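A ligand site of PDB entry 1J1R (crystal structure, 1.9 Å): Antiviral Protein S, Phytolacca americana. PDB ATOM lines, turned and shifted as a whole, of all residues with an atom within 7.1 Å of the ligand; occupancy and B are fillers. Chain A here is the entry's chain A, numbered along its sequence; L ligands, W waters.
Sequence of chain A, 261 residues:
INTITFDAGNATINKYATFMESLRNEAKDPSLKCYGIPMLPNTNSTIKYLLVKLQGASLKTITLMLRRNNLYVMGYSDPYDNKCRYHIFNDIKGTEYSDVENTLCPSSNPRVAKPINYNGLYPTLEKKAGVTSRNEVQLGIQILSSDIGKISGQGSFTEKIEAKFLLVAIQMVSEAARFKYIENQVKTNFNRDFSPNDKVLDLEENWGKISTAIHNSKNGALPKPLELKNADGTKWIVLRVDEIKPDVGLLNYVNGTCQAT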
ATOM      1  N   LEU A  66      27.691  16.084 -15.748  1.00  0.00           N
ATOM      2  CA  LEU A  66      28.073  15.008 -14.834  1.00  0.00           C
ATOM      3  C   LEU A  66      27.481  15.132 -13.438  1.00  0.00           C
ATOM      4  O   LEU A  66      27.477  16.228 -12.871  1.00  0.00           O
ATOM      5  CB  LEU A  66      29.586  14.918 -14.608  1.00  0.00           C
ATOM      6  CG  LEU A  66      30.526  14.307 -15.624  1.00  0.00           C
ATOM      7  CD1 LEU A  66      30.252  14.973 -16.945  1.00  0.00           C
ATOM      8  CD2 LEU A  66      31.981  14.534 -15.264  1.00  0.00           C
ATOM      9  N   ASN A  70      29.147  10.647  -8.489  1.00  0.00           N
ATOM     10  CA  ASN A  70      29.793   9.461  -9.012  1.00  0.00           C
ATOM     11  C   ASN A  70      30.336   9.675 -10.402  1.00  0.00           C
ATOM     12  O   ASN A  70      30.707   8.689 -11.019  1.00  0.00           O
ATOM     13  CB  ASN A  70      28.778   8.298  -9.002  1.00  0.00           C
ATOM     14  CG  ASN A  70      27.548   8.576  -9.838  1.00  0.00           C
ATOM     15  OD1 ASN A  70      27.373   9.650 -10.413  1.00  0.00           O
ATOM     16  ND2 ASN A  70      26.684   7.593  -9.975  1.00  0.00           N
ATOM     17  N   LEU A  71      30.367  10.962 -10.862  1.00  0.00           N
ATOM     18  CA  LEU A  71      30.857  11.359 -12.173  1.00  0.00           C
ATOM     19  C   LEU A  71      30.138  10.767 -13.384  1.00  0.00           C
ATOM     20  O   LEU A  71      30.684  10.622 -14.472  1.00  0.00           O
ATOM     21  CB  LEU A  71      32.357  11.064 -12.250  1.00  0.00           C
ATOM     22  CG  LEU A  71      33.210  11.963 -11.400  1.00  0.00           C
ATOM     23  CD1 LEU A  71      34.632  11.492 -11.476  1.00  0.00           C
ATOM     24  CD2 LEU A  71      33.108  13.398 -11.910  1.00  0.00           C
ATOM     25  N   TYR A  72      28.859  10.434 -13.236  1.00  0.00           N
ATOM     26  CA  TYR A  72      28.080   9.885 -14.344  1.00  0.00           C
ATOM     27  C   TYR A  72      27.644  10.973 -15.309  1.00  0.00           C
ATOM     28  O   TYR A  72      27.176  12.022 -14.860  1.00  0.00           O
ATOM     29  CB  TYR A  72      26.828   9.162 -13.862  1.00  0.00           C
ATOM     30  CG  TYR A  72      27.047   7.685 -13.913  1.00  0.00           C
ATOM     31  CD1 TYR A  72      26.370   6.884 -14.802  1.00  0.00           C
ATOM     32  CD2 TYR A  72      28.005   7.150 -13.054  1.00  0.00           C
ATOM     33  CE1 TYR A  72      26.659   5.536 -14.834  1.00  0.00           C
ATOM     34  CE2 TYR A  72      28.295   5.784 -13.086  1.00  0.00           C
ATOM     35  CZ  TYR A  72      27.628   4.983 -13.985  1.00  0.00           C
ATOM     36  OH  TYR A  72      27.983   3.635 -14.073  1.00  0.00           O
ATOM     37  N   VAL A  73      27.808  10.729 -16.616  1.00  0.00           N
ATOM     38  CA  VAL A  73      27.278  11.638 -17.635  1.00  0.00           C
ATOM     39  C   VAL A  73      25.767  11.395 -17.706  1.00  0.00           C
ATOM     40  O   VAL A  73      25.307  10.286 -17.914  1.00  0.00           O
ATOM     41  CB  VAL A  73      28.003  11.365 -19.032  1.00  0.00           C
ATOM     42  CG1 VAL A  73      27.443  12.187 -20.215  1.00  0.00           C
ATOM     43  CG2 VAL A  73      29.471  11.705 -18.829  1.00  0.00           C
ATOM     44  N   MET A  74      24.962  12.455 -17.463  1.00  0.00           N
ATOM     45  CA  MET A  74      23.496  12.449 -17.514  1.00  0.00           C
ATOM     46  C   MET A  74      22.886  12.851 -18.854  1.00  0.00           C
ATOM     47  O   MET A  74      21.758  12.495 -19.152  1.00  0.00           O
ATOM     48  CB  MET A  74      22.958  13.400 -16.488  1.00  0.00           C
ATOM     49  CG  MET A  74      23.474  12.931 -15.155  1.00  0.00           C
ATOM     50  SD  MET A  74      23.079  14.120 -13.887  1.00  0.00           S
ATOM     51  CE  MET A  74      21.606  13.188 -13.517  1.00  0.00           C
ATOM     52  N   PHE A  89      19.528  11.171 -21.345  1.00  0.00           N
ATOM     53  CA  PHE A  89      19.219   9.732 -21.351  1.00  0.00           C
ATOM     54  C   PHE A  89      17.792   9.414 -20.942  1.00  0.00           C
ATOM     55  O   PHE A  89      17.233  10.144 -20.121  1.00  0.00           O
ATOM     56  CB  PHE A  89      20.218   9.028 -20.445  1.00  0.00           C
ATOM     57  CG  PHE A  89      21.616   8.915 -21.061  1.00  0.00           C
ATOM     58  CD1 PHE A  89      21.803   8.195 -22.241  1.00  0.00           C
ATOM     59  CD2 PHE A  89      22.703   9.501 -20.431  1.00  0.00           C
ATOM     60  CE1 PHE A  89      23.065   8.077 -22.782  1.00  0.00           C
ATOM     61  CE2 PHE A  89      23.970   9.371 -20.987  1.00  0.00           C
ATOM     62  CZ  PHE A  89      24.145   8.668 -22.158  1.00  0.00           C
ATOM     63  N   ASN A 119      19.528   4.404 -22.356  1.00  0.00           N
ATOM     64  CA  ASN A 119      20.190   4.788 -21.126  1.00  0.00           C
ATOM     65  C   ASN A 119      21.721   4.820 -21.279  1.00  0.00           C
ATOM     66  O   ASN A 119      22.251   4.402 -22.313  1.00  0.00           O
ATOM     67  CB  ASN A 119      19.798   3.835 -19.978  1.00  0.00           C
ATOM     68  CG  ASN A 119      20.193   2.363 -20.064  1.00  0.00           C
ATOM     69  OD1 ASN A 119      19.358   1.482 -19.832  1.00  0.00           O
ATOM     70  ND2 ASN A 119      21.426   2.009 -20.365  1.00  0.00           N
ATOM     71  N   GLY A 120      22.434   5.269 -20.222  1.00  0.00           N
ATOM     72  CA  GLY A 120      23.861   5.472 -20.265  1.00  0.00           C
ATOM     73  C   GLY A 120      24.737   4.335 -19.774  1.00  0.00           C
ATOM     74  O   GLY A 120      25.882   4.595 -19.476  1.00  0.00           O
ATOM     75  N   LEU A 121      24.273   3.093 -19.680  1.00  0.00           N
ATOM     76  CA  LEU A 121      25.062   1.964 -19.224  1.00  0.00           C
ATOM     77  C   LEU A 121      25.883   1.415 -20.400  1.00  0.00           C
ATOM     78  O   LEU A 121      25.464   1.456 -21.541  1.00  0.00           O
ATOM     79  CB  LEU A 121      24.126   0.884 -18.659  1.00  0.00           C
ATOM     80  CG  LEU A 121      23.138   1.260 -17.539  1.00  0.00           C
ATOM     81  CD1 LEU A 121      22.198   0.098 -17.300  1.00  0.00           C
ATOM     82  CD2 LEU A 121      23.901   1.666 -16.280  1.00  0.00           C
ATOM     83  N   TYR A 122      27.090   0.926 -20.084  1.00  0.00           N
ATOM     84  CA  TYR A 122      27.997   0.377 -21.078  1.00  0.00           C
ATOM     85  C   TYR A 122      27.430  -0.693 -21.978  1.00  0.00           C
ATOM     86  O   TYR A 122      27.720  -0.626 -23.151  1.00  0.00           O
ATOM     87  CB  TYR A 122      29.309  -0.187 -20.391  1.00  0.00           C
ATOM     88  CG  TYR A 122      30.355   0.877 -20.022  1.00  0.00           C
ATOM     89  CD1 TYR A 122      30.570   1.946 -20.891  1.00  0.00           C
ATOM     90  CD2 TYR A 122      31.101   0.774 -18.845  1.00  0.00           C
ATOM     91  CE1 TYR A 122      31.510   2.906 -20.583  1.00  0.00           C
ATOM     92  CE2 TYR A 122      32.046   1.722 -18.552  1.00  0.00           C
ATOM     93  CZ  TYR A 122      32.249   2.774 -19.424  1.00  0.00           C
ATOM     94  OH  TYR A 122      33.202   3.710 -19.185  1.00  0.00           O
ATOM     95  N   PRO A 123      26.611  -1.672 -21.539  1.00  0.00           N
ATOM     96  CA  PRO A 123      26.020  -2.680 -22.429  1.00  0.00           C
ATOM     97  C   PRO A 123      25.074  -2.112 -23.461  1.00  0.00           C
ATOM     98  O   PRO A 123      25.070  -2.543 -24.609  1.00  0.00           O
ATOM     99  CB  PRO A 123      25.370  -3.650 -21.442  1.00  0.00           C
ATOM    100  CG  PRO A 123      26.171  -3.530 -20.166  1.00  0.00           C
ATOM    101  CD  PRO A 123      26.331  -2.018 -20.121  1.00  0.00           C
ATOM    102  N   LEU A 125      25.270   1.167 -24.547  1.00  0.00           N
ATOM    103  CA  LEU A 125      26.015   1.960 -25.514  1.00  0.00           C
ATOM    104  C   LEU A 125      26.817   1.099 -26.493  1.00  0.00           C
ATOM    105  O   LEU A 125      27.015   1.512 -27.642  1.00  0.00           O
ATOM    106  CB  LEU A 125      26.960   2.911 -24.788  1.00  0.00           C
ATOM    107  CG  LEU A 125      26.427   3.948 -23.812  1.00  0.00           C
ATOM    108  CD1 LEU A 125      27.605   4.556 -23.091  1.00  0.00           C
ATOM    109  CD2 LEU A 125      25.645   4.990 -24.524  1.00  0.00           C
ATOM    110  N   LEU A 166      29.834   8.860 -27.113  1.00  0.00           N
ATOM    111  CA  LEU A 166      29.677   8.770 -25.675  1.00  0.00           C
ATOM    112  C   LEU A 166      30.580   7.702 -25.084  1.00  0.00           C
ATOM    113  O   LEU A 166      31.050   7.949 -23.971  1.00  0.00           O
ATOM    114  CB  LEU A 166      28.225   8.466 -25.348  1.00  0.00           C
ATOM    115  CG  LEU A 166      27.227   9.571 -25.663  1.00  0.00           C
ATOM    116  CD1 LEU A 166      25.810   9.019 -25.694  1.00  0.00           C
ATOM    117  CD2 LEU A 166      27.366  10.644 -24.635  1.00  0.00           C
ATOM    118  N   ILE A 170      33.005   9.302 -22.210  1.00  0.00           N
ATOM    119  CA  ILE A 170      32.884   8.784 -20.857  1.00  0.00           C
ATOM    120  C   ILE A 170      34.239   8.231 -20.433  1.00  0.00           C
ATOM    121  O   ILE A 170      34.626   8.546 -19.306  1.00  0.00           O
ATOM    122  CB  ILE A 170      31.819   7.665 -20.755  1.00  0.00           C
ATOM    123  CG1 ILE A 170      30.413   8.230 -20.922  1.00  0.00           C
ATOM    124  CG2 ILE A 170      31.929   7.013 -19.394  1.00  0.00           C
ATOM    125  CD1 ILE A 170      29.327   7.192 -21.259  1.00  0.00           C
ATOM    126  N   GLN A 171      34.979   7.518 -21.284  1.00  0.00           N
ATOM    127  CA  GLN A 171      36.249   6.950 -20.864  1.00  0.00           C
ATOM    128  C   GLN A 171      37.390   7.977 -20.771  1.00  0.00           C
ATOM    129  O   GLN A 171      38.202   7.899 -19.833  1.00  0.00           O
ATOM    130  CB  GLN A 171      36.613   5.828 -21.833  1.00  0.00           C
ATOM    131  CG  GLN A 171      35.596   4.702 -21.685  1.00  0.00           C
ATOM    132  CD  GLN A 171      35.775   3.494 -22.612  1.00  0.00           C
ATOM    133  OE1 GLN A 171      36.348   2.477 -22.218  1.00  0.00           O
ATOM    134  NE2 GLN A 171      35.298   3.551 -23.848  1.00  0.00           N
ATOM    135  N   SER A 174      35.257  10.939 -17.560  1.00  0.00           N
ATOM    136  CA  SER A 174      34.899  10.264 -16.310  1.00  0.00           C
ATOM    137  C   SER A 174      35.832   9.125 -15.901  1.00  0.00           C
ATOM    138  O   SER A 174      36.314   9.176 -14.782  1.00  0.00           O
ATOM    139  CB  SER A 174      33.469   9.727 -16.382  1.00  0.00           C
ATOM    140  OG  SER A 174      32.563  10.802 -16.325  1.00  0.00           O
ATOM    141  N   GLU A 175      36.135   8.110 -16.725  1.00  0.00           N
ATOM    142  CA  GLU A 175      37.030   7.025 -16.330  1.00  0.00           C
ATOM    143  C   GLU A 175      38.469   7.444 -16.130  1.00  0.00           C
ATOM    144  O   GLU A 175      39.120   6.920 -15.251  1.00  0.00           O
ATOM    145  CB  GLU A 175      37.037   5.903 -17.338  1.00  0.00           C
ATOM    146  CG  GLU A 175      35.681   5.237 -17.535  1.00  0.00           C
ATOM    147  CD  GLU A 175      35.145   4.398 -16.389  1.00  0.00           C
ATOM    148  OE1 GLU A 175      35.567   4.514 -15.234  1.00  0.00           O
ATOM    149  OE2 GLU A 175      34.261   3.594 -16.690  1.00  0.00           O
ATOM    150  N   ARG A 178      38.632   9.068 -12.664  1.00  0.00           N
ATOM    151  CA  ARG A 178      38.507   8.079 -11.634  1.00  0.00           C
ATOM    152  C   ARG A 178      39.812   7.318 -11.509  1.00  0.00           C
ATOM    153  O   ARG A 178      40.293   7.102 -10.399  1.00  0.00           O
ATOM    154  CB  ARG A 178      37.409   7.127 -11.985  1.00  0.00           C
ATOM    155  CG  ARG A 178      36.034   7.671 -11.948  1.00  0.00           C
ATOM    156  CD  ARG A 178      35.105   6.638 -12.505  1.00  0.00           C
ATOM    157  NE  ARG A 178      33.729   7.101 -12.434  1.00  0.00           N
ATOM    158  CZ  ARG A 178      32.842   6.880 -13.446  1.00  0.00           C
ATOM    159  NH1 ARG A 178      33.202   6.224 -14.553  1.00  0.00           N
ATOM    160  NH2 ARG A 178      31.582   7.354 -13.371  1.00  0.00           N
ATOM    161  N   GLU A 204      37.555  -0.078 -14.936  1.00  0.00           N
ATOM    162  CA  GLU A 204      36.275   0.591 -15.152  1.00  0.00           C
ATOM    163  C   GLU A 204      35.115  -0.089 -14.440  1.00  0.00           C
ATOM    164  O   GLU A 204      34.318   0.540 -13.739  1.00  0.00           O
ATOM    165  CB  GLU A 204      35.949   0.663 -16.644  1.00  0.00           C
ATOM    166  CG  GLU A 204      36.868   1.599 -17.403  1.00  0.00           C
ATOM    167  CD  GLU A 204      36.715   1.634 -18.928  1.00  0.00           C
ATOM    168  OE1 GLU A 204      36.162   0.711 -19.508  1.00  0.00           O
ATOM    169  OE2 GLU A 204      37.194   2.565 -19.570  1.00  0.00           O
HETATM  170  N1  LIG L   1      30.196   4.261 -16.902  1.00  0.00           N
HETATM  171  C1  LIG L   1      29.112   3.667 -17.422  1.00  0.00           C
HETATM  172  N2  LIG L   1      28.257   4.515 -17.912  1.00  0.00           N
HETATM  173  C2  LIG L   1      28.775   5.767 -17.558  1.00  0.00           C
HETATM  174  C3  LIG L   1      28.277   7.085 -17.701  1.00  0.00           C
HETATM  175  N3  LIG L   1      27.100   7.367 -18.317  1.00  0.00           N
HETATM  176  N4  LIG L   1      28.996   8.059 -17.104  1.00  0.00           N
HETATM  177  C4  LIG L   1      30.092   7.730 -16.441  1.00  0.00           C
HETATM  178  N5  LIG L   1      30.666   6.552 -16.275  1.00  0.00           N
HETATM  179  C5  LIG L   1      29.929   5.600 -16.868  1.00  0.00           C
HETATM  180  O   HOH W   1      31.866   2.886 -15.285  1.00  0.00           O
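Merely in contact with the ligand: Leu 71 (3.5 Å), Tyr 72 (3.4 Å), Tyr 122 (3.5 Å), Ile 170 (3.4 Å) and Ser 174 (3.9 Å).
Of the 20 residues printed, 8 come within 4 Å of the ligand.
The nearest printed residue that does not touch the ligand is Glu 175 (4.1 Å).
N of Tyr 72 lies close to OD1 of Asn 70 (3.3 Å).
The backbone carbonyl oxygen of Leu 71 lies within hydrogen-bond range of the side-chain hydroxyl of Ser 174 (2.6 Å).
The guanidinium group (NH2) of Arg 178 sits at hydrogen-bond distance from the backbone carbonyl oxygen (O) of Asn 70, 2.8 Å away.
The guanidinium group (NH1) of Arg 178 lies within salt-bridge range of the side-chain carboxylate (OE1) of Glu 175, 3.0 Å away.
OH of Tyr 122 is in hydrogen-bond range of OE2 of Glu 175, 2.7 Å away.
The backbone carbonyl oxygen of Ile 170 sits at hydrogen-bond distance from the backbone NH of Glu 175, at 3.0 Å.
Water W1 lies within hydrogen-bond range of N1 of the ligand (2.7 Å) and OE2 of Glu 175 (2.9 Å).
A nitrogen (N3) of the ligand lies within hydrogen-bond range of the backbone carbonyl oxygen (O) of Gly 120.
A nitrogen (N3) of the ligand is in hydrogen-bond range of the backbone carbonyl oxygen (O) of Val 73, at 3.4 Å.
A nitrogen (N5) of the ligand sits at hydrogen-bond distance from the guanidinium group of Arg 178, 3.1 Å away.
A nitrogen (N4) of the ligand sits at hydrogen-bond distance from the backbone NH (N) of Val 73 (3.0 Å).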
